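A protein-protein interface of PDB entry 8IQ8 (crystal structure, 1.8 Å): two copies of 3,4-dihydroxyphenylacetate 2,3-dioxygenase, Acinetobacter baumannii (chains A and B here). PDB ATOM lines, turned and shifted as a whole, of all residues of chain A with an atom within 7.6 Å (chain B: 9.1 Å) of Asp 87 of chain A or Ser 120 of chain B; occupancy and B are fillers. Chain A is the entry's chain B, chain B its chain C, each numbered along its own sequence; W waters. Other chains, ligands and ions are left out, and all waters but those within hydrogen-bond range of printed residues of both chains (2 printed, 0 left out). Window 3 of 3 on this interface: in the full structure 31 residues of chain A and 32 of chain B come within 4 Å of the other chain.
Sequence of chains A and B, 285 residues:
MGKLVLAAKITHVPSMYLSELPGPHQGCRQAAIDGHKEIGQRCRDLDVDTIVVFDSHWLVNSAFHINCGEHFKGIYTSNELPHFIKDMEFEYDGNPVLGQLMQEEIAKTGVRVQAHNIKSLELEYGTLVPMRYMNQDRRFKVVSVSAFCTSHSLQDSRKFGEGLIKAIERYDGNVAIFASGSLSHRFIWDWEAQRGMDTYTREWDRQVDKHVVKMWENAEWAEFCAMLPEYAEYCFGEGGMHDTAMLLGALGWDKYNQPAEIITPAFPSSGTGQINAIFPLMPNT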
ATOM      1  N   TYR A  17       3.365 -20.324  20.045  1.00  0.00           N
ATOM      2  CA  TYR A  17       4.621 -19.767  19.459  1.00  0.00           C
ATOM      3  C   TYR A  17       5.223 -18.736  20.435  1.00  0.00           C
ATOM      4  O   TYR A  17       6.417 -18.822  20.711  1.00  0.00           O
ATOM      5  CB  TYR A  17       4.406 -19.192  18.061  1.00  0.00           C
ATOM      6  CG  TYR A  17       5.675 -18.739  17.378  1.00  0.00           C
ATOM      7  CD1 TYR A  17       6.147 -17.446  17.530  1.00  0.00           C
ATOM      8  CD2 TYR A  17       6.394 -19.599  16.573  1.00  0.00           C
ATOM      9  CE1 TYR A  17       7.294 -17.020  16.888  1.00  0.00           C
ATOM     10  CE2 TYR A  17       7.565 -19.197  15.946  1.00  0.00           C
ATOM     11  CZ  TYR A  17       8.012 -17.894  16.095  1.00  0.00           C
ATOM     12  OH  TYR A  17       9.158 -17.462  15.490  1.00  0.00           O
ATOM     13  N   GLY A  74       7.227 -22.535   2.569  1.00  0.00           N
ATOM     14  CA  GLY A  74       7.258 -21.068   2.560  1.00  0.00           C
ATOM     15  C   GLY A  74       7.696 -20.489   3.884  1.00  0.00           C
ATOM     16  O   GLY A  74       8.327 -21.209   4.694  1.00  0.00           O
ATOM     17  N   ILE A  75       7.344 -19.217   4.065  1.00  0.00           N
ATOM     18  CA  ILE A  75       7.723 -18.339   5.201  1.00  0.00           C
ATOM     19  C   ILE A  75       6.413 -17.733   5.685  1.00  0.00           C
ATOM     20  O   ILE A  75       5.662 -17.186   4.841  1.00  0.00           O
ATOM     21  CB  ILE A  75       8.754 -17.281   4.752  1.00  0.00           C
ATOM     22  CG1 ILE A  75       9.783 -17.844   3.767  1.00  0.00           C
ATOM     23  CG2 ILE A  75       9.430 -16.652   5.952  1.00  0.00           C
ATOM     24  CD1 ILE A  75      10.675 -18.926   4.352  1.00  0.00           C
ATOM     25  N   TYR A  76       6.071 -17.962   6.947  1.00  0.00           N
ATOM     26  CA  TYR A  76       4.777 -17.544   7.522  1.00  0.00           C
ATOM     27  C   TYR A  76       4.976 -16.292   8.389  1.00  0.00           C
ATOM     28  O   TYR A  76       5.734 -16.341   9.360  1.00  0.00           O
ATOM     29  CB  TYR A  76       4.140 -18.674   8.331  1.00  0.00           C
ATOM     30  CG  TYR A  76       2.852 -18.217   8.957  1.00  0.00           C
ATOM     31  CD1 TYR A  76       2.845 -17.698  10.235  1.00  0.00           C
ATOM     32  CD2 TYR A  76       1.666 -18.202   8.232  1.00  0.00           C
ATOM     33  CE1 TYR A  76       1.687 -17.190  10.797  1.00  0.00           C
ATOM     34  CE2 TYR A  76       0.487 -17.721   8.791  1.00  0.00           C
ATOM     35  CZ  TYR A  76       0.513 -17.182  10.067  1.00  0.00           C
ATOM     36  OH  TYR A  76      -0.615 -16.690  10.650  1.00  0.00           O
ATOM     37  N   THR A  77       4.237 -15.226   8.094  1.00  0.00           N
ATOM     38  CA  THR A  77       4.086 -14.048   8.978  1.00  0.00           C
ATOM     39  C   THR A  77       2.616 -13.911   9.355  1.00  0.00           C
ATOM     40  O   THR A  77       1.794 -13.787   8.439  1.00  0.00           O
ATOM     41  CB  THR A  77       4.674 -12.791   8.329  1.00  0.00           C
ATOM     42  OG1 THR A  77       6.086 -12.969   8.292  1.00  0.00           O
ATOM     43  CG2 THR A  77       4.350 -11.526   9.089  1.00  0.00           C
ATOM     44  N   SER A  78       2.311 -13.945  10.653  1.00  0.00           N
ATOM     45  CA  SER A  78       0.944 -13.732  11.184  1.00  0.00           C
ATOM     46  C   SER A  78       0.460 -12.328  10.821  1.00  0.00           C
ATOM     47  O   SER A  78       1.210 -11.334  11.056  1.00  0.00           O
ATOM     48  CB  SER A  78       0.886 -13.924  12.650  1.00  0.00           C
ATOM     49  OG  SER A  78      -0.405 -13.591  13.158  1.00  0.00           O
ATOM     50  N   ASN A  79      -0.772 -12.215  10.347  1.00  0.00           N
ATOM     51  CA  ASN A  79      -1.387 -10.875  10.187  1.00  0.00           C
ATOM     52  C   ASN A  79      -2.155 -10.524  11.470  1.00  0.00           C
ATOM     53  O   ASN A  79      -2.704  -9.429  11.504  1.00  0.00           O
ATOM     54  CB  ASN A  79      -2.182 -10.768   8.887  1.00  0.00           C
ATOM     55  CG  ASN A  79      -3.247 -11.820   8.762  1.00  0.00           C
ATOM     56  OD1 ASN A  79      -3.566 -12.509   9.737  1.00  0.00           O
ATOM     57  ND2 ASN A  79      -3.777 -11.965   7.553  1.00  0.00           N
ATOM     58  N   PRO A  82       2.033  -9.721  13.977  1.00  0.00           N
ATOM     59  CA  PRO A  82       3.194  -9.734  13.100  1.00  0.00           C
ATOM     60  C   PRO A  82       4.493  -9.267  13.774  1.00  0.00           C
ATOM     61  O   PRO A  82       5.554  -9.595  13.258  1.00  0.00           O
ATOM     62  CB  PRO A  82       2.774  -8.818  11.948  1.00  0.00           C
ATOM     63  CG  PRO A  82       1.741  -7.908  12.550  1.00  0.00           C
ATOM     64  CD  PRO A  82       1.023  -8.726  13.599  1.00  0.00           C
ATOM     65  N   PHE A  84       5.554 -10.398  16.649  1.00  0.00           N
ATOM     66  CA  PHE A  84       6.078 -11.608  17.342  1.00  0.00           C
ATOM     67  C   PHE A  84       6.188 -12.826  16.400  1.00  0.00           C
ATOM     68  O   PHE A  84       7.167 -13.580  16.503  1.00  0.00           O
ATOM     69  CB  PHE A  84       5.186 -11.903  18.546  1.00  0.00           C
ATOM     70  CG  PHE A  84       5.243 -10.864  19.643  1.00  0.00           C
ATOM     71  CD1 PHE A  84       6.342 -10.777  20.488  1.00  0.00           C
ATOM     72  CD2 PHE A  84       4.184  -9.993  19.849  1.00  0.00           C
ATOM     73  CE1 PHE A  84       6.383  -9.832  21.511  1.00  0.00           C
ATOM     74  CE2 PHE A  84       4.216  -9.058  20.880  1.00  0.00           C
ATOM     75  CZ  PHE A  84       5.321  -8.971  21.705  1.00  0.00           C
ATOM     76  N   ILE A  85       5.196 -13.069  15.541  1.00  0.00           N
ATOM     77  CA  ILE A  85       5.142 -14.287  14.671  1.00  0.00           C
ATOM     78  C   ILE A  85       5.401 -13.862  13.223  1.00  0.00           C
ATOM     79  O   ILE A  85       4.450 -13.427  12.527  1.00  0.00           O
ATOM     80  CB  ILE A  85       3.810 -15.040  14.827  1.00  0.00           C
ATOM     81  CG1 ILE A  85       3.416 -15.219  16.295  1.00  0.00           C
ATOM     82  CG2 ILE A  85       3.881 -16.380  14.094  1.00  0.00           C
ATOM     83  CD1 ILE A  85       2.030 -15.830  16.490  1.00  0.00           C
ATOM     84  N   LYS A  86       6.650 -13.982  12.786  1.00  0.00           N
ATOM     85  CA  LYS A  86       7.083 -13.484  11.465  1.00  0.00           C
ATOM     86  C   LYS A  86       8.266 -14.317  10.972  1.00  0.00           C
ATOM     87  O   LYS A  86       9.019 -14.852  11.818  1.00  0.00           O
ATOM     88  CB  LYS A  86       7.422 -11.994  11.573  1.00  0.00           C
ATOM     89  CG  LYS A  86       8.429 -11.660  12.668  1.00  0.00           C
ATOM     90  CD  LYS A  86       8.926 -10.235  12.563  1.00  0.00           C
ATOM     91  CE  LYS A  86       9.715  -9.803  13.783  1.00  0.00           C
ATOM     92  NZ  LYS A  86       9.701  -8.326  13.916  1.00  0.00           N
ATOM     93  N   ASP A  87       8.375 -14.432   9.651  1.00  0.00           N
ATOM     94  CA  ASP A  87       9.513 -15.065   8.941  1.00  0.00           C
ATOM     95  C   ASP A  87       9.662 -16.502   9.460  1.00  0.00           C
ATOM     96  O   ASP A  87      10.789 -16.976   9.582  1.00  0.00           O
ATOM     97  CB  ASP A  87      10.755 -14.178   9.084  1.00  0.00           C
ATOM     98  CG  ASP A  87      10.494 -12.740   8.635  1.00  0.00           C
ATOM     99  OD1 ASP A  87      10.093 -12.561   7.469  1.00  0.00           O
ATOM    100  OD2 ASP A  87      10.623 -11.824   9.478  1.00  0.00           O
ATOM    101  N   MET A  88       8.547 -17.167   9.770  1.00  0.00           N
ATOM    102  CA  MET A  88       8.552 -18.553  10.309  1.00  0.00           C
ATOM    103  C   MET A  88       8.615 -19.537   9.134  1.00  0.00           C
ATOM    104  O   MET A  88       7.592 -19.687   8.438  1.00  0.00           O
ATOM    105  CB  MET A  88       7.308 -18.837  11.156  1.00  0.00           C
ATOM    106  CG  MET A  88       7.301 -20.242  11.718  1.00  0.00           C
ATOM    107  SD  MET A  88       5.836 -20.598  12.725  1.00  0.00           S
ATOM    108  CE  MET A  88       4.650 -21.037  11.459  1.00  0.00           C
ATOM    109  N   GLU A  89       9.787 -20.126   8.909  1.00  0.00           N
ATOM    110  CA  GLU A  89      10.059 -21.176   7.890  1.00  0.00           C
ATOM    111  C   GLU A  89       9.253 -22.453   8.167  1.00  0.00           C
ATOM    112  O   GLU A  89       9.144 -22.858   9.337  1.00  0.00           O
ATOM    113  CB  GLU A  89      11.536 -21.575   7.889  1.00  0.00           C
ATOM    114  CG  GLU A  89      12.440 -20.593   7.168  1.00  0.00           C
ATOM    115  CD  GLU A  89      13.892 -21.043   7.095  1.00  0.00           C
ATOM    116  OE1 GLU A  89      14.332 -21.834   7.977  1.00  0.00           O
ATOM    117  OE2 GLU A  89      14.577 -20.626   6.139  1.00  0.00           O
ATOM    118  N   PHE A  90       8.780 -23.098   7.100  1.00  0.00           N
ATOM    119  CA  PHE A  90       8.119 -24.428   7.142  1.00  0.00           C
ATOM    120  C   PHE A  90       8.285 -25.149   5.798  1.00  0.00           C
ATOM    121  O   PHE A  90       8.365 -24.484   4.731  1.00  0.00           O
ATOM    122  CB  PHE A  90       6.639 -24.286   7.502  1.00  0.00           C
ATOM    123  CG  PHE A  90       5.800 -23.620   6.442  1.00  0.00           C
ATOM    124  CD1 PHE A  90       5.297 -24.340   5.366  1.00  0.00           C
ATOM    125  CD2 PHE A  90       5.519 -22.263   6.513  1.00  0.00           C
ATOM    126  CE1 PHE A  90       4.534 -23.719   4.391  1.00  0.00           C
ATOM    127  CE2 PHE A  90       4.750 -21.649   5.536  1.00  0.00           C
ATOM    128  CZ  PHE A  90       4.275 -22.375   4.465  1.00  0.00           C
ATOM    129  N   ASN B  67      -0.401  -1.648   8.205  1.00  0.00           N
ATOM    130  CA  ASN B  67       0.641  -2.156   7.275  1.00  0.00           C
ATOM    131  C   ASN B  67       1.191  -0.943   6.526  1.00  0.00           C
ATOM    132  O   ASN B  67       0.565  -0.531   5.549  1.00  0.00           O
ATOM    133  CB  ASN B  67       0.115  -3.219   6.315  1.00  0.00           C
ATOM    134  CG  ASN B  67       1.246  -3.922   5.575  1.00  0.00           C
ATOM    135  OD1 ASN B  67       2.351  -3.400   5.482  1.00  0.00           O
ATOM    136  ND2 ASN B  67       1.004  -5.123   5.105  1.00  0.00           N
ATOM    137  N   GLY B  69       4.458  -0.915   5.329  1.00  0.00           N
ATOM    138  CA  GLY B  69       5.685  -1.478   4.731  1.00  0.00           C
ATOM    139  C   GLY B  69       6.196  -0.560   3.643  1.00  0.00           C
ATOM    140  O   GLY B  69       5.383   0.144   3.059  1.00  0.00           O
ATOM    141  N   GLU B  70       7.512  -0.543   3.418  1.00  0.00           N
ATOM    142  CA  GLU B  70       8.184   0.357   2.443  1.00  0.00           C
ATOM    143  C   GLU B  70       7.772  -0.035   1.024  1.00  0.00           C
ATOM    144  O   GLU B  70       7.511   0.830   0.209  1.00  0.00           O
ATOM    145  CB  GLU B  70       9.706   0.244   2.596  1.00  0.00           C
ATOM    146  CG  GLU B  70      10.489   0.960   1.502  1.00  0.00           C
ATOM    147  CD  GLU B  70      10.542   2.465   1.666  1.00  0.00           C
ATOM    148  OE1 GLU B  70      10.658   2.920   2.823  1.00  0.00           O
ATOM    149  OE2 GLU B  70      10.478   3.184   0.643  1.00  0.00           O
ATOM    150  N   HIS B  71       7.765  -1.327   0.738  1.00  0.00           N
ATOM    151  CA  HIS B  71       7.546  -1.862  -0.628  1.00  0.00           C
ATOM    152  C   HIS B  71       6.728  -3.154  -0.524  1.00  0.00           C
ATOM    153  O   HIS B  71       7.021  -3.958   0.369  1.00  0.00           O
ATOM    154  CB  HIS B  71       8.902  -2.039  -1.333  1.00  0.00           C
ATOM    155  CG  HIS B  71       8.777  -2.321  -2.789  1.00  0.00           C
ATOM    156  ND1 HIS B  71       8.575  -1.315  -3.724  1.00  0.00           N
ATOM    157  CD2 HIS B  71       8.821  -3.484  -3.478  1.00  0.00           C
ATOM    158  CE1 HIS B  71       8.503  -1.857  -4.926  1.00  0.00           C
ATOM    159  NE2 HIS B  71       8.646  -3.184  -4.800  1.00  0.00           N
ATOM    160  N   PHE B  72       5.732  -3.316  -1.401  1.00  0.00           N
ATOM    161  CA  PHE B  72       4.850  -4.509  -1.465  1.00  0.00           C
ATOM    162  C   PHE B  72       5.006  -5.153  -2.841  1.00  0.00           C
ATOM    163  O   PHE B  72       4.673  -4.507  -3.834  1.00  0.00           O
ATOM    164  CB  PHE B  72       3.389  -4.116  -1.238  1.00  0.00           C
ATOM    165  CG  PHE B  72       3.122  -3.290  -0.006  1.00  0.00           C
ATOM    166  CD1 PHE B  72       3.192  -3.852   1.259  1.00  0.00           C
ATOM    167  CD2 PHE B  72       2.747  -1.960  -0.105  1.00  0.00           C
ATOM    168  CE1 PHE B  72       2.926  -3.098   2.390  1.00  0.00           C
ATOM    169  CE2 PHE B  72       2.488  -1.202   1.026  1.00  0.00           C
ATOM    170  CZ  PHE B  72       2.571  -1.774   2.275  1.00  0.00           C
ATOM    171  N   LYS B  73       5.535  -6.364  -2.900  1.00  0.00           N
ATOM    172  CA  LYS B  73       5.677  -7.117  -4.171  1.00  0.00           C
ATOM    173  C   LYS B  73       5.370  -8.589  -3.905  1.00  0.00           C
ATOM    174  O   LYS B  73       5.945  -9.172  -2.967  1.00  0.00           O
ATOM    175  CB  LYS B  73       7.078  -6.943  -4.770  1.00  0.00           C
ATOM    176  CG  LYS B  73       7.270  -7.595  -6.139  1.00  0.00           C
ATOM    177  CD  LYS B  73       8.726  -7.750  -6.490  1.00  0.00           C
ATOM    178  CE  LYS B  73       8.960  -8.703  -7.642  1.00  0.00           C
ATOM    179  NZ  LYS B  73       8.653  -8.055  -8.934  1.00  0.00           N
ATOM    180  N   HIS B 116       3.462  -1.492  11.363  1.00  0.00           N
ATOM    181  CA  HIS B 116       4.349  -2.584  10.893  1.00  0.00           C
ATOM    182  C   HIS B 116       4.985  -2.214   9.562  1.00  0.00           C
ATOM    183  O   HIS B 116       4.261  -1.915   8.581  1.00  0.00           O
ATOM    184  CB  HIS B 116       3.578  -3.885  10.742  1.00  0.00           C
ATOM    185  CG  HIS B 116       2.819  -4.245  11.964  1.00  0.00           C
ATOM    186  ND1 HIS B 116       3.442  -4.667  13.115  1.00  0.00           N
ATOM    187  CD2 HIS B 116       1.501  -4.222  12.221  1.00  0.00           C
ATOM    188  CE1 HIS B 116       2.536  -4.894  14.035  1.00  0.00           C
ATOM    189  NE2 HIS B 116       1.332  -4.655  13.501  1.00  0.00           N
ATOM    190  N   ASN B 117       6.302  -2.270   9.549  1.00  0.00           N
ATOM    191  CA  ASN B 117       7.130  -2.130   8.327  1.00  0.00           C
ATOM    192  C   ASN B 117       7.938  -3.415   8.201  1.00  0.00           C
ATOM    193  O   ASN B 117       9.133  -3.395   8.580  1.00  0.00           O
ATOM    194  CB  ASN B 117       7.987  -0.865   8.392  1.00  0.00           C
ATOM    195  CG  ASN B 117       8.766  -0.621   7.121  1.00  0.00           C
ATOM    196  OD1 ASN B 117       8.627  -1.362   6.153  1.00  0.00           O
ATOM    197  ND2 ASN B 117       9.599   0.407   7.126  1.00  0.00           N
ATOM    198  N   ILE B 118       7.289  -4.465   7.681  1.00  0.00           N
ATOM    199  CA  ILE B 118       7.815  -5.864   7.593  1.00  0.00           C
ATOM    200  C   ILE B 118       7.634  -6.359   6.151  1.00  0.00           C
ATOM    201  O   ILE B 118       6.469  -6.474   5.724  1.00  0.00           O
ATOM    202  CB  ILE B 118       7.051  -6.777   8.576  1.00  0.00           C
ATOM    203  CG1 ILE B 118       7.087  -6.282  10.022  1.00  0.00           C
ATOM    204  CG2 ILE B 118       7.532  -8.213   8.463  1.00  0.00           C
ATOM    205  CD1 ILE B 118       6.055  -6.949  10.907  1.00  0.00           C
ATOM    206  N   LYS B 119       8.727  -6.673   5.439  1.00  0.00           N
ATOM    207  CA  LYS B 119       8.697  -7.173   4.035  1.00  0.00           C
ATOM    208  C   LYS B 119       7.683  -8.327   3.905  1.00  0.00           C
ATOM    209  O   LYS B 119       6.925  -8.340   2.923  1.00  0.00           O
ATOM    210  CB  LYS B 119      10.079  -7.677   3.594  1.00  0.00           C
ATOM    211  CG  LYS B 119      11.181  -6.639   3.451  1.00  0.00           C
ATOM    212  CD  LYS B 119      12.461  -7.223   2.840  1.00  0.00           C
ATOM    213  CE  LYS B 119      13.521  -6.187   2.508  1.00  0.00           C
ATOM    214  NZ  LYS B 119      13.680  -5.201   3.605  1.00  0.00           N
ATOM    215  N   SER B 120       7.664  -9.257   4.868  1.00  0.00           N
ATOM    216  CA  SER B 120       6.870 -10.512   4.809  1.00  0.00           C
ATOM    217  C   SER B 120       5.417 -10.319   5.279  1.00  0.00           C
ATOM    218  O   SER B 120       4.656 -11.303   5.168  1.00  0.00           O
ATOM    219  CB  SER B 120       7.561 -11.627   5.569  1.00  0.00           C
ATOM    220  OG  SER B 120       7.545 -11.400   6.972  1.00  0.00           O
ATOM    221  N   LEU B 121       5.015  -9.128   5.757  1.00  0.00           N
ATOM    222  CA  LEU B 121       3.586  -8.838   6.070  1.00  0.00           C
ATOM    223  C   LEU B 121       2.932  -8.323   4.784  1.00  0.00           C
ATOM    224  O   LEU B 121       3.160  -7.157   4.429  1.00  0.00           O
ATOM    225  CB  LEU B 121       3.428  -7.822   7.204  1.00  0.00           C
ATOM    226  CG  LEU B 121       1.969  -7.602   7.617  1.00  0.00           C
ATOM    227  CD1 LEU B 121       1.370  -8.883   8.193  1.00  0.00           C
ATOM    228  CD2 LEU B 121       1.820  -6.452   8.578  1.00  0.00           C
ATOM    229  N   GLU B 122       2.202  -9.196   4.092  1.00  0.00           N
ATOM    230  CA  GLU B 122       1.695  -8.951   2.720  1.00  0.00           C
ATOM    231  C   GLU B 122       0.395  -8.145   2.809  1.00  0.00           C
ATOM    232  O   GLU B 122      -0.312  -8.248   3.823  1.00  0.00           O
ATOM    233  CB  GLU B 122       1.470 -10.283   2.001  1.00  0.00           C
ATOM    234  CG  GLU B 122       2.731 -11.134   1.863  1.00  0.00           C
ATOM    235  CD  GLU B 122       3.798 -10.577   0.934  1.00  0.00           C
ATOM    236  OE1 GLU B 122       3.433  -9.870  -0.037  1.00  0.00           O
ATOM    237  OE2 GLU B 122       5.010 -10.864   1.171  1.00  0.00           O
ATOM    238  N   LEU B 123       0.097  -7.373   1.769  1.00  0.00           N
ATOM    239  CA  LEU B 123      -1.190  -6.654   1.622  1.00  0.00           C
ATOM    240  C   LEU B 123      -2.342  -7.664   1.602  1.00  0.00           C
ATOM    241  O   LEU B 123      -2.232  -8.700   0.912  1.00  0.00           O
ATOM    242  CB  LEU B 123      -1.182  -5.838   0.332  1.00  0.00           C
ATOM    243  CG  LEU B 123      -0.332  -4.565   0.332  1.00  0.00           C
ATOM    244  CD1 LEU B 123      -0.464  -3.863  -1.000  1.00  0.00           C
ATOM    245  CD2 LEU B 123      -0.725  -3.620   1.455  1.00  0.00           C
ATOM    246  N   GLU B 124      -3.417  -7.368   2.343  1.00  0.00           N
ATOM    247  CA  GLU B 124      -4.671  -8.169   2.357  1.00  0.00           C
ATOM    248  C   GLU B 124      -5.544  -7.804   1.148  1.00  0.00           C
ATOM    249  O   GLU B 124      -5.289  -6.758   0.493  1.00  0.00           O
ATOM    250  CB  GLU B 124      -5.458  -7.972   3.655  1.00  0.00           C
ATOM    251  CG  GLU B 124      -5.372  -9.167   4.590  1.00  0.00           C
ATOM    252  CD  GLU B 124      -3.946  -9.540   4.919  1.00  0.00           C
ATOM    253  OE1 GLU B 124      -3.055  -8.897   4.353  1.00  0.00           O
ATOM    254  OE2 GLU B 124      -3.728 -10.457   5.732  1.00  0.00           O
HETATM  255  O   HOH W   1       1.171 -12.039   5.804  1.00  0.00           O
HETATM  256  O   HOH W   2      10.191  -9.693   6.584  1.00  0.00           O
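O of Ser 78 of chain A touches CD1 of Leu 121 of chain B (3.8 Å).
Leu 121 of chain B touches Asn 79 of chain A.
His 116 of chain B touches Pro 82 of chain A (NE2 to CG, 3.4 Å).
O of Pro 82 of chain A touches CD1 of Ile 118 of chain B, 3.6 Å away.
The side-chain hydroxyl of Thr 77 of chain A sits at hydrogen-bond distance from the side-chain hydroxyl of Ser 120 of chain B (2.5 Å).
The side-chain amide nitrogen of Asn 79 of chain A sits close to the side-chain carboxylate of Glu 124 of chain B, at 2.4 Å.
The side-chain carboxylate (OD1) of Asp 87 of chain A sits at hydrogen-bond distance from the side-chain hydroxyl (OG) of Ser 120 of chain B (2.8 Å).
The side-chain amide nitrogen (ND2) of Asn 67 of chain B is in hydrogen-bond range of the backbone carbonyl oxygen (O) of Leu 121 of chain B (3.0 Å).
The backbone carbonyl oxygen of Ile 85 of chain A is in hydrogen-bond range of the backbone NH of Ser 78 of chain A.
The backbone carbonyl oxygen (O) of His 116 of chain B sits at hydrogen-bond distance from the backbone NH (N) of Gly 69 of chain B.
N of Asp 87 of chain A sits at hydrogen-bond distance from O of Tyr 76 of chain A, 3.3 Å away.
The side-chain hydroxyl of Thr 77 of chain A is in hydrogen-bond range of the backbone NH of Asp 87 of chain A, 3.0 Å away.
Of the 15 printed residues of chain B, 5 touch a printed residue of chain A.
Printed residues of chain B that touch a printed residue of chain A: His 116, Ile 118, Ser 120, Leu 121 and Glu 124.
Hydrophobic or aromatic side chains of chain A that line the printed part of chain B: Pro 82.
Among the printed residues, 7 pairs touch across the chains.
No position is printed for both chains.
Printed residues of chain A within 4 Å of Ser 120 of chain B: Thr 77 and Asp 87.
Of the printed residues of chain B, Pro 82 of chain A touches His 116 and Ile 118.
Printed residues of chain B within 4 Å of Ser 78 of chain A: Leu 121.
Of the printed residues of chain A, Ile 118 of chain B touches Pro 82.
Printed residues of chain B within 4 Å of Asn 79 of chain A: Leu 121 and Glu 124.
Gly 74 of chain A touches none of the printed residues of chain B.
Tyr 76 of chain A touches none of the printed residues of chain B.
The nearest residue of chain B that does not touch Asp 87 of chain A is Ile 118 of chain B (4.9 Å).
The nearest residue of chain A that does not touch Ser 120 of chain B is Lys 86 of chain A (4.6 Å).
The nearest printed residue of chain A that does not touch Ile 118 of chain B is Thr 77 of chain A (4.6 Å).
Water W2 bridges OD1 of Asp 87 of chain A (3.0 Å) and N of Ser 120 of chain B (3.1 Å).
Water W1 bridges O of Thr 77 of chain A (3.2 Å) and N of Glu 122 of chain B (3.5 Å).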
